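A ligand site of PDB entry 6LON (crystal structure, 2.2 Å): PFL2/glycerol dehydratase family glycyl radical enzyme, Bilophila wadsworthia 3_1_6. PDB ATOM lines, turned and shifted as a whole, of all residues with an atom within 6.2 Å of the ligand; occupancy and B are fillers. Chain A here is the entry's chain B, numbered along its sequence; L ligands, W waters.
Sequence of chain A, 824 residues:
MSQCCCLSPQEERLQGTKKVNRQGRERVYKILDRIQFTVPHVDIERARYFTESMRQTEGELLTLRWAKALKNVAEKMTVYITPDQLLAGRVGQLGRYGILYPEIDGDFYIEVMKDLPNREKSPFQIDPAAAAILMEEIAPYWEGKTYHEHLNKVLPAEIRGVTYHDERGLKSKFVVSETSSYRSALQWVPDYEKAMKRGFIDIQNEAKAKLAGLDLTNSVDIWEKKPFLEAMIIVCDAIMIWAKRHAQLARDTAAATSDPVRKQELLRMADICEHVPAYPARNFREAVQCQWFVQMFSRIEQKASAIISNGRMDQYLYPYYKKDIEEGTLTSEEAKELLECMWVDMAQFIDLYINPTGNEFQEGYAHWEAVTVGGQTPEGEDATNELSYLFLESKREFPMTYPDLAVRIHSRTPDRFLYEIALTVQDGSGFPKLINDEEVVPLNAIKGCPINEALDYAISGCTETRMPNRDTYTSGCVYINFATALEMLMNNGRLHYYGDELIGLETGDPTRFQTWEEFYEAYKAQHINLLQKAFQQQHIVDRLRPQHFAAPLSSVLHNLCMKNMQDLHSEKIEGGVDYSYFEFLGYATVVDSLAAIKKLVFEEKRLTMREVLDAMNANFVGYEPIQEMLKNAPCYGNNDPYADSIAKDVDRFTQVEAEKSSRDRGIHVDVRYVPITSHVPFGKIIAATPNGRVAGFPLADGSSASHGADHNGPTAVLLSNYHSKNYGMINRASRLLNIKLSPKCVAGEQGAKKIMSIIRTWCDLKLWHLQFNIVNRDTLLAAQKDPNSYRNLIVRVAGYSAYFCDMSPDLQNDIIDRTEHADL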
ATOM      1  N   ARG A 183       8.657  34.069  11.518  1.00  0.00           N
ATOM      2  CA  ARG A 183       7.798  33.539  12.573  1.00  0.00           C
ATOM      3  C   ARG A 183       7.675  34.635  13.621  1.00  0.00           C
ATOM      4  O   ARG A 183       8.518  35.509  13.717  1.00  0.00           O
ATOM      5  CB  ARG A 183       8.343  32.244  13.169  1.00  0.00           C
ATOM      6  CG  ARG A 183       9.845  32.294  13.485  1.00  0.00           C
ATOM      7  CD  ARG A 183      10.402  31.026  14.052  1.00  0.00           C
ATOM      8  NE  ARG A 183      11.881  31.091  14.188  1.00  0.00           N
ATOM      9  CZ  ARG A 183      12.588  30.273  14.963  1.00  0.00           C
ATOM     10  NH1 ARG A 183      11.986  29.322  15.684  1.00  0.00           N
ATOM     11  NH2 ARG A 183      13.921  30.375  15.038  1.00  0.00           N
ATOM     12  N   ALA A 185       7.689  34.119  16.874  1.00  0.00           N
ATOM     13  CA  ALA A 185       8.201  33.717  18.175  1.00  0.00           C
ATOM     14  C   ALA A 185       8.707  32.305  18.043  1.00  0.00           C
ATOM     15  O   ALA A 185       8.376  31.604  17.079  1.00  0.00           O
ATOM     16  CB  ALA A 185       7.125  33.768  19.242  1.00  0.00           C
ATOM     17  N   LEU A 186       9.512  31.884  19.025  1.00  0.00           N
ATOM     18  CA  LEU A 186       9.821  30.497  19.195  1.00  0.00           C
ATOM     19  C   LEU A 186       8.539  29.707  19.402  1.00  0.00           C
ATOM     20  O   LEU A 186       7.433  30.264  19.532  1.00  0.00           O
ATOM     21  CB  LEU A 186      10.717  30.299  20.406  1.00  0.00           C
ATOM     22  CG  LEU A 186      12.112  30.917  20.345  1.00  0.00           C
ATOM     23  CD1 LEU A 186      12.676  31.104  21.736  1.00  0.00           C
ATOM     24  CD2 LEU A 186      12.993  29.989  19.504  1.00  0.00           C
ATOM     25  N   GLN A 187       8.693  28.385  19.461  1.00  0.00           N
ATOM     26  CA  GLN A 187       7.587  27.514  19.857  1.00  0.00           C
ATOM     27  C   GLN A 187       7.070  27.921  21.245  1.00  0.00           C
ATOM     28  O   GLN A 187       7.775  28.561  22.013  1.00  0.00           O
ATOM     29  CB  GLN A 187       8.012  26.039  19.852  1.00  0.00           C
ATOM     30  CG  GLN A 187       9.405  25.695  20.352  1.00  0.00           C
ATOM     31  CD  GLN A 187       9.688  26.172  21.781  1.00  0.00           C
ATOM     32  OE1 GLN A 187       8.815  26.145  22.649  1.00  0.00           O
ATOM     33  NE2 GLN A 187      10.928  26.591  22.032  1.00  0.00           N
ATOM     34  N   SER A 305       6.541  29.348  16.587  1.00  0.00           N
ATOM     35  CA  SER A 305       7.287  28.429  15.737  1.00  0.00           C
ATOM     36  C   SER A 305       6.746  27.010  15.877  1.00  0.00           C
ATOM     37  O   SER A 305       6.441  26.546  16.977  1.00  0.00           O
ATOM     38  CB  SER A 305       8.773  28.437  16.062  1.00  0.00           C
ATOM     39  OG  SER A 305       9.507  27.968  14.951  1.00  0.00           O
ATOM     40  N   ALA A 306       6.637  26.327  14.741  1.00  0.00           N
ATOM     41  CA  ALA A 306       6.288  24.921  14.633  1.00  0.00           C
ATOM     42  C   ALA A 306       4.773  24.725  14.679  1.00  0.00           C
ATOM     43  O   ALA A 306       4.294  23.576  14.546  1.00  0.00           O
ATOM     44  CB  ALA A 306       6.962  24.078  15.732  1.00  0.00           C
ATOM     45  N   GLN A 362      11.729  25.110   6.702  1.00  0.00           N
ATOM     46  CA  GLN A 362      10.633  24.224   7.035  1.00  0.00           C
ATOM     47  C   GLN A 362       9.930  23.718   5.776  1.00  0.00           C
ATOM     48  O   GLN A 362       8.704  23.800   5.654  1.00  0.00           O
ATOM     49  CB  GLN A 362       9.649  24.905   7.993  1.00  0.00           C
ATOM     50  CG  GLN A 362      10.020  24.869   9.482  1.00  0.00           C
ATOM     51  CD  GLN A 362      10.634  26.177  10.027  1.00  0.00           C
ATOM     52  OE1 GLN A 362      10.762  26.366  11.242  1.00  0.00           O
ATOM     53  NE2 GLN A 362      10.972  27.085   9.130  1.00  0.00           N
ATOM     54  N   TRP A 368       5.443  20.861  13.928  1.00  0.00           N
ATOM     55  CA  TRP A 368       5.695  20.026  15.110  1.00  0.00           C
ATOM     56  C   TRP A 368       4.813  20.548  16.246  1.00  0.00           C
ATOM     57  O   TRP A 368       5.288  21.216  17.184  1.00  0.00           O
ATOM     58  CB  TRP A 368       7.146  20.025  15.557  1.00  0.00           C
ATOM     59  CG  TRP A 368       8.195  19.677  14.580  1.00  0.00           C
ATOM     60  CD1 TRP A 368       8.849  18.465  14.459  1.00  0.00           C
ATOM     61  CD2 TRP A 368       8.807  20.555  13.632  1.00  0.00           C
ATOM     62  NE1 TRP A 368       9.811  18.557  13.488  1.00  0.00           N
ATOM     63  CE2 TRP A 368       9.800  19.812  12.951  1.00  0.00           C
ATOM     64  CE3 TRP A 368       8.597  21.883  13.271  1.00  0.00           C
ATOM     65  CZ2 TRP A 368      10.576  20.357  11.942  1.00  0.00           C
ATOM     66  CZ3 TRP A 368       9.365  22.421  12.252  1.00  0.00           C
ATOM     67  CH2 TRP A 368      10.350  21.670  11.605  1.00  0.00           C
ATOM     68  N   SER A 460       7.870  20.826  23.330  1.00  0.00           N
ATOM     69  CA  SER A 460       7.361  21.930  22.526  1.00  0.00           C
ATOM     70  C   SER A 460       8.126  21.971  21.216  1.00  0.00           C
ATOM     71  O   SER A 460       9.370  21.957  21.204  1.00  0.00           O
ATOM     72  CB  SER A 460       7.472  23.259  23.273  1.00  0.00           C
ATOM     73  OG  SER A 460       6.749  24.279  22.614  1.00  0.00           O
ATOM     74  N   GLY A 461       7.402  22.039  20.114  1.00  0.00           N
ATOM     75  CA  GLY A 461       8.066  22.081  18.831  1.00  0.00           C
ATOM     76  C   GLY A 461       8.792  20.772  18.560  1.00  0.00           C
ATOM     77  O   GLY A 461       8.313  19.683  18.907  1.00  0.00           O
ATOM     78  N   CYS A 462       9.991  20.884  18.008  1.00  0.00           N
ATOM     79  CA  CYS A 462      10.739  19.706  17.598  1.00  0.00           C
ATOM     80  C   CYS A 462      11.307  18.941  18.796  1.00  0.00           C
ATOM     81  O   CYS A 462      11.151  17.724  18.890  1.00  0.00           O
ATOM     82  CB  CYS A 462      11.857  20.117  16.629  1.00  0.00           C
ATOM     83  SG  CYS A 462      12.778  18.747  15.964  1.00  0.00           S
ATOM     84  N   THR A 463      11.989  19.635  19.719  1.00  0.00           N
ATOM     85  CA  THR A 463      12.591  18.971  20.874  1.00  0.00           C
ATOM     86  C   THR A 463      12.653  19.848  22.108  1.00  0.00           C
ATOM     87  O   THR A 463      13.314  19.468  23.089  1.00  0.00           O
ATOM     88  CB  THR A 463      14.008  18.477  20.537  1.00  0.00           C
ATOM     89  OG1 THR A 463      14.764  19.536  19.955  1.00  0.00           O
ATOM     90  CG2 THR A 463      13.930  17.307  19.550  1.00  0.00           C
ATOM     91  N   GLU A 464      11.955  20.959  22.131  1.00  0.00           N
ATOM     92  CA  GLU A 464      12.206  21.941  23.167  1.00  0.00           C
ATOM     93  C   GLU A 464      11.341  21.621  24.377  1.00  0.00           C
ATOM     94  O   GLU A 464      10.466  20.759  24.334  1.00  0.00           O
ATOM     95  CB  GLU A 464      11.984  23.339  22.612  1.00  0.00           C
ATOM     96  CG  GLU A 464      13.094  23.777  21.664  1.00  0.00           C
ATOM     97  CD  GLU A 464      13.631  22.642  20.752  1.00  0.00           C
ATOM     98  OE1 GLU A 464      12.979  22.303  19.719  1.00  0.00           O
ATOM     99  OE2 GLU A 464      14.682  22.083  21.098  1.00  0.00           O
ATOM    100  N   ARG A 466       9.310  23.364  27.600  1.00  0.00           N
ATOM    101  CA  ARG A 466       8.679  24.582  28.077  1.00  0.00           C
ATOM    102  C   ARG A 466       8.074  24.353  29.448  1.00  0.00           C
ATOM    103  O   ARG A 466       7.486  23.306  29.729  1.00  0.00           O
ATOM    104  CB  ARG A 466       7.580  25.078  27.114  1.00  0.00           C
ATOM    105  CG  ARG A 466       8.118  25.788  25.886  1.00  0.00           C
ATOM    106  CD  ARG A 466       8.856  27.061  26.212  1.00  0.00           C
ATOM    107  NE  ARG A 466       9.062  27.842  25.009  1.00  0.00           N
ATOM    108  CZ  ARG A 466       9.629  29.053  24.979  1.00  0.00           C
ATOM    109  NH1 ARG A 466      10.084  29.632  26.089  1.00  0.00           N
ATOM    110  NH2 ARG A 466       9.764  29.651  23.831  1.00  0.00           N
ATOM    111  N   GLY A 476      13.013  33.893  18.133  1.00  0.00           N
ATOM    112  CA  GLY A 476      13.575  32.928  17.204  1.00  0.00           C
ATOM    113  C   GLY A 476      15.050  33.158  17.034  1.00  0.00           C
ATOM    114  O   GLY A 476      15.473  34.312  16.866  1.00  0.00           O
ATOM    115  N   CYS A 477      15.846  32.100  17.088  1.00  0.00           N
ATOM    116  CA  CYS A 477      17.282  32.242  17.244  1.00  0.00           C
ATOM    117  C   CYS A 477      18.051  31.856  15.974  1.00  0.00           C
ATOM    118  O   CYS A 477      17.605  31.070  15.129  1.00  0.00           O
ATOM    119  CB  CYS A 477      17.783  31.423  18.454  1.00  0.00           C
ATOM    120  SG  CYS A 477      17.513  32.335  20.011  1.00  0.00           S
ATOM    121  N   TYR A 479      20.618  30.602  13.102  1.00  0.00           N
ATOM    122  CA  TYR A 479      21.076  29.314  12.585  1.00  0.00           C
ATOM    123  C   TYR A 479      22.453  29.503  11.936  1.00  0.00           C
ATOM    124  O   TYR A 479      22.617  30.329  11.038  1.00  0.00           O
ATOM    125  CB  TYR A 479      20.072  28.757  11.558  1.00  0.00           C
ATOM    126  CG  TYR A 479      19.005  27.876  12.181  1.00  0.00           C
ATOM    127  CD1 TYR A 479      18.192  28.352  13.210  1.00  0.00           C
ATOM    128  CD2 TYR A 479      18.847  26.558  11.788  1.00  0.00           C
ATOM    129  CE1 TYR A 479      17.282  27.536  13.828  1.00  0.00           C
ATOM    130  CE2 TYR A 479      17.914  25.733  12.380  1.00  0.00           C
ATOM    131  CZ  TYR A 479      17.131  26.223  13.415  1.00  0.00           C
ATOM    132  OH  TYR A 479      16.213  25.401  14.023  1.00  0.00           O
ATOM    133  N   TYR A 581      19.002  30.251  22.348  1.00  0.00           N
ATOM    134  CA  TYR A 581      19.618  29.218  21.541  1.00  0.00           C
ATOM    135  C   TYR A 581      20.493  29.835  20.468  1.00  0.00           C
ATOM    136  O   TYR A 581      20.408  31.019  20.151  1.00  0.00           O
ATOM    137  CB  TYR A 581      18.572  28.334  20.860  1.00  0.00           C
ATOM    138  CG  TYR A 581      17.530  27.764  21.780  1.00  0.00           C
ATOM    139  CD1 TYR A 581      17.868  26.807  22.738  1.00  0.00           C
ATOM    140  CD2 TYR A 581      16.203  28.173  21.697  1.00  0.00           C
ATOM    141  CE1 TYR A 581      16.923  26.264  23.572  1.00  0.00           C
ATOM    142  CE2 TYR A 581      15.238  27.641  22.542  1.00  0.00           C
ATOM    143  CZ  TYR A 581      15.621  26.690  23.488  1.00  0.00           C
ATOM    144  OH  TYR A 581      14.655  26.152  24.316  1.00  0.00           O
ATOM    145  N   GLU A 583      21.884  27.680  16.707  1.00  0.00           N
ATOM    146  CA  GLU A 583      21.880  26.369  16.042  1.00  0.00           C
ATOM    147  C   GLU A 583      23.222  26.043  15.398  1.00  0.00           C
ATOM    148  O   GLU A 583      23.785  26.834  14.636  1.00  0.00           O
ATOM    149  CB  GLU A 583      20.794  26.282  14.956  1.00  0.00           C
ATOM    150  CG  GLU A 583      20.031  24.979  15.107  1.00  0.00           C
ATOM    151  CD  GLU A 583      19.123  25.024  16.333  1.00  0.00           C
ATOM    152  OE1 GLU A 583      18.460  26.070  16.516  1.00  0.00           O
ATOM    153  OE2 GLU A 583      19.110  24.025  17.098  1.00  0.00           O
ATOM    154  N   ARG A 672      22.579  24.468  20.459  1.00  0.00           N
ATOM    155  CA  ARG A 672      21.510  23.532  20.152  1.00  0.00           C
ATOM    156  C   ARG A 672      21.767  22.939  18.783  1.00  0.00           C
ATOM    157  O   ARG A 672      22.320  23.614  17.914  1.00  0.00           O
ATOM    158  CB  ARG A 672      20.131  24.219  20.170  1.00  0.00           C
ATOM    159  CG  ARG A 672      18.932  23.272  20.276  1.00  0.00           C
ATOM    160  CD  ARG A 672      17.610  24.060  20.347  1.00  0.00           C
ATOM    161  NE  ARG A 672      17.272  24.718  19.104  1.00  0.00           N
ATOM    162  CZ  ARG A 672      16.124  25.324  18.879  1.00  0.00           C
ATOM    163  NH1 ARG A 672      15.195  25.367  19.838  1.00  0.00           N
ATOM    164  NH2 ARG A 672      15.906  25.888  17.694  1.00  0.00           N
ATOM    165  N   VAL A 674      19.285  21.377  16.488  1.00  0.00           N
ATOM    166  CA  VAL A 674      17.937  21.136  15.997  1.00  0.00           C
ATOM    167  C   VAL A 674      17.859  21.706  14.583  1.00  0.00           C
ATOM    168  O   VAL A 674      17.652  22.913  14.415  1.00  0.00           O
ATOM    169  CB  VAL A 674      16.867  21.793  16.878  1.00  0.00           C
ATOM    170  CG1 VAL A 674      15.435  21.647  16.265  1.00  0.00           C
ATOM    171  CG2 VAL A 674      16.904  21.234  18.280  1.00  0.00           C
ATOM    172  N   ILE A 676      15.819  21.532  11.856  1.00  0.00           N
ATOM    173  CA  ILE A 676      14.628  21.581  10.991  1.00  0.00           C
ATOM    174  C   ILE A 676      15.092  21.123   9.601  1.00  0.00           C
ATOM    175  O   ILE A 676      15.801  20.114   9.511  1.00  0.00           O
ATOM    176  CB  ILE A 676      13.947  22.958  11.040  1.00  0.00           C
ATOM    177  CG1 ILE A 676      14.934  24.121  10.849  1.00  0.00           C
ATOM    178  CG2 ILE A 676      13.230  23.119  12.387  1.00  0.00           C
ATOM    179  CD1 ILE A 676      14.279  25.497  11.098  1.00  0.00           C
HETATM  180  C1  LIG L   1      11.516  25.532  16.903  1.00  0.00           C
HETATM  181  O1  LIG L   1      13.510  27.370  17.479  1.00  0.00           O
HETATM  182  C2  LIG L   1      12.036  24.120  17.015  1.00  0.00           C
HETATM  183  O2  LIG L   1      12.529  26.110  19.468  1.00  0.00           O
HETATM  184  C3  LIG L   1      11.725  23.533  15.650  1.00  0.00           C
HETATM  185  O3  LIG L   1      11.177  27.708  18.181  1.00  0.00           O
HETATM  186  S1  LIG L   1      12.279  26.683  18.093  1.00  0.00           S
HETATM  187  O4  LIG L   1      11.359  23.454  18.044  1.00  0.00           O
HETATM  188  O5  LIG L   1      10.341  23.550  15.460  1.00  0.00           O
HETATM  189  O   HOH W   1       9.506  25.305  13.684  1.00  0.00           O
HETATM  190  O   HOH W   2      15.653  29.194  17.099  1.00  0.00           O
HETATM  191  O   HOH W   3      13.855  26.524  14.781  1.00  0.00           O
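The backbone NH (N) of Cys 462 sits at hydrogen-bond distance from an oxygen (O4) of the ligand, 2.9 Å away.
An oxygen (O4) of the ligand lies within hydrogen-bond range of the side-chain carboxylate of Glu 464.
O2 of the ligand lies within salt-bridge range of NH1 of Arg 672 (2.8 Å).
The side-chain amide nitrogen of Gln 187 sits at hydrogen-bond distance from an oxygen (O2) of the ligand, at 3.1 Å.
O1 of the ligand is in salt-bridge range of NH1 of Arg 183, at 3.1 Å.
N of Gln 187 sits at hydrogen-bond distance from O3 of the ligand (2.9 Å).
N of Trp 368 is in hydrogen-bond range of O of Ala 306.
The side-chain carboxylate (OE2) of Glu 583 lies within salt-bridge range of the guanidinium group (NE) of Arg 672, 2.8 Å away.
The backbone carbonyl oxygen of Leu 186 is in hydrogen-bond range of the backbone NH of Ser 305 (3.2 Å).
The guanidinium group (NH1) of Arg 183 lies within hydrogen-bond range of the side-chain hydroxyl (OG) of Ser 305 (2.9 Å).
NH2 of Arg 466 sits at hydrogen-bond distance from O of Gln 187, at 2.9 Å.
The side-chain carboxylate of Glu 464 sits at hydrogen-bond distance from the side-chain hydroxyl of Thr 463 (2.8 Å).
The backbone carbonyl oxygen of Ala 185 lies within hydrogen-bond range of the backbone NH of Ser 305 (2.9 Å).
The side-chain hydroxyl (OG) of Ser 460 sits at hydrogen-bond distance from the side-chain amide oxygen (OE1) of Gln 187.
CD2 of Leu 186 touches O3 of the ligand, at 3.2 Å.
Ser 305 touches the ligand (CB to O3, 3.3 Å).
CB of Ala 306 touches O5 of the ligand, 3.4 Å away.
Trp 368 touches the ligand (CE3 to O5, 3.3 Å).
Gly 461 touches the ligand (CA to O4, 3.7 Å).
Ile 676 touches the ligand (CG2 to C3, 3.6 Å).
Hydrophobic or aromatic side chains that line the ligand: Leu 186, Ala 306, Trp 368 and Ile 676.
11 residues have an atom within 4 Å of the ligand: Arg 183, Leu 186, Gln 187, Ser 305, Ala 306, Trp 368, Gly 461, Cys 462, Glu 464, Arg 672 and Ile 676.
The nearest printed residue that does not touch the ligand is Ser 460 (4.02 Å).
Water W1 lies within hydrogen-bond range of O5 of the ligand, OE1 of Gln 362, OG of Ser 305 and N of Ala 306.
Water W3 lies within hydrogen-bond range of OH of Tyr 479, O1 of the ligand and NH1 of Arg 183.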
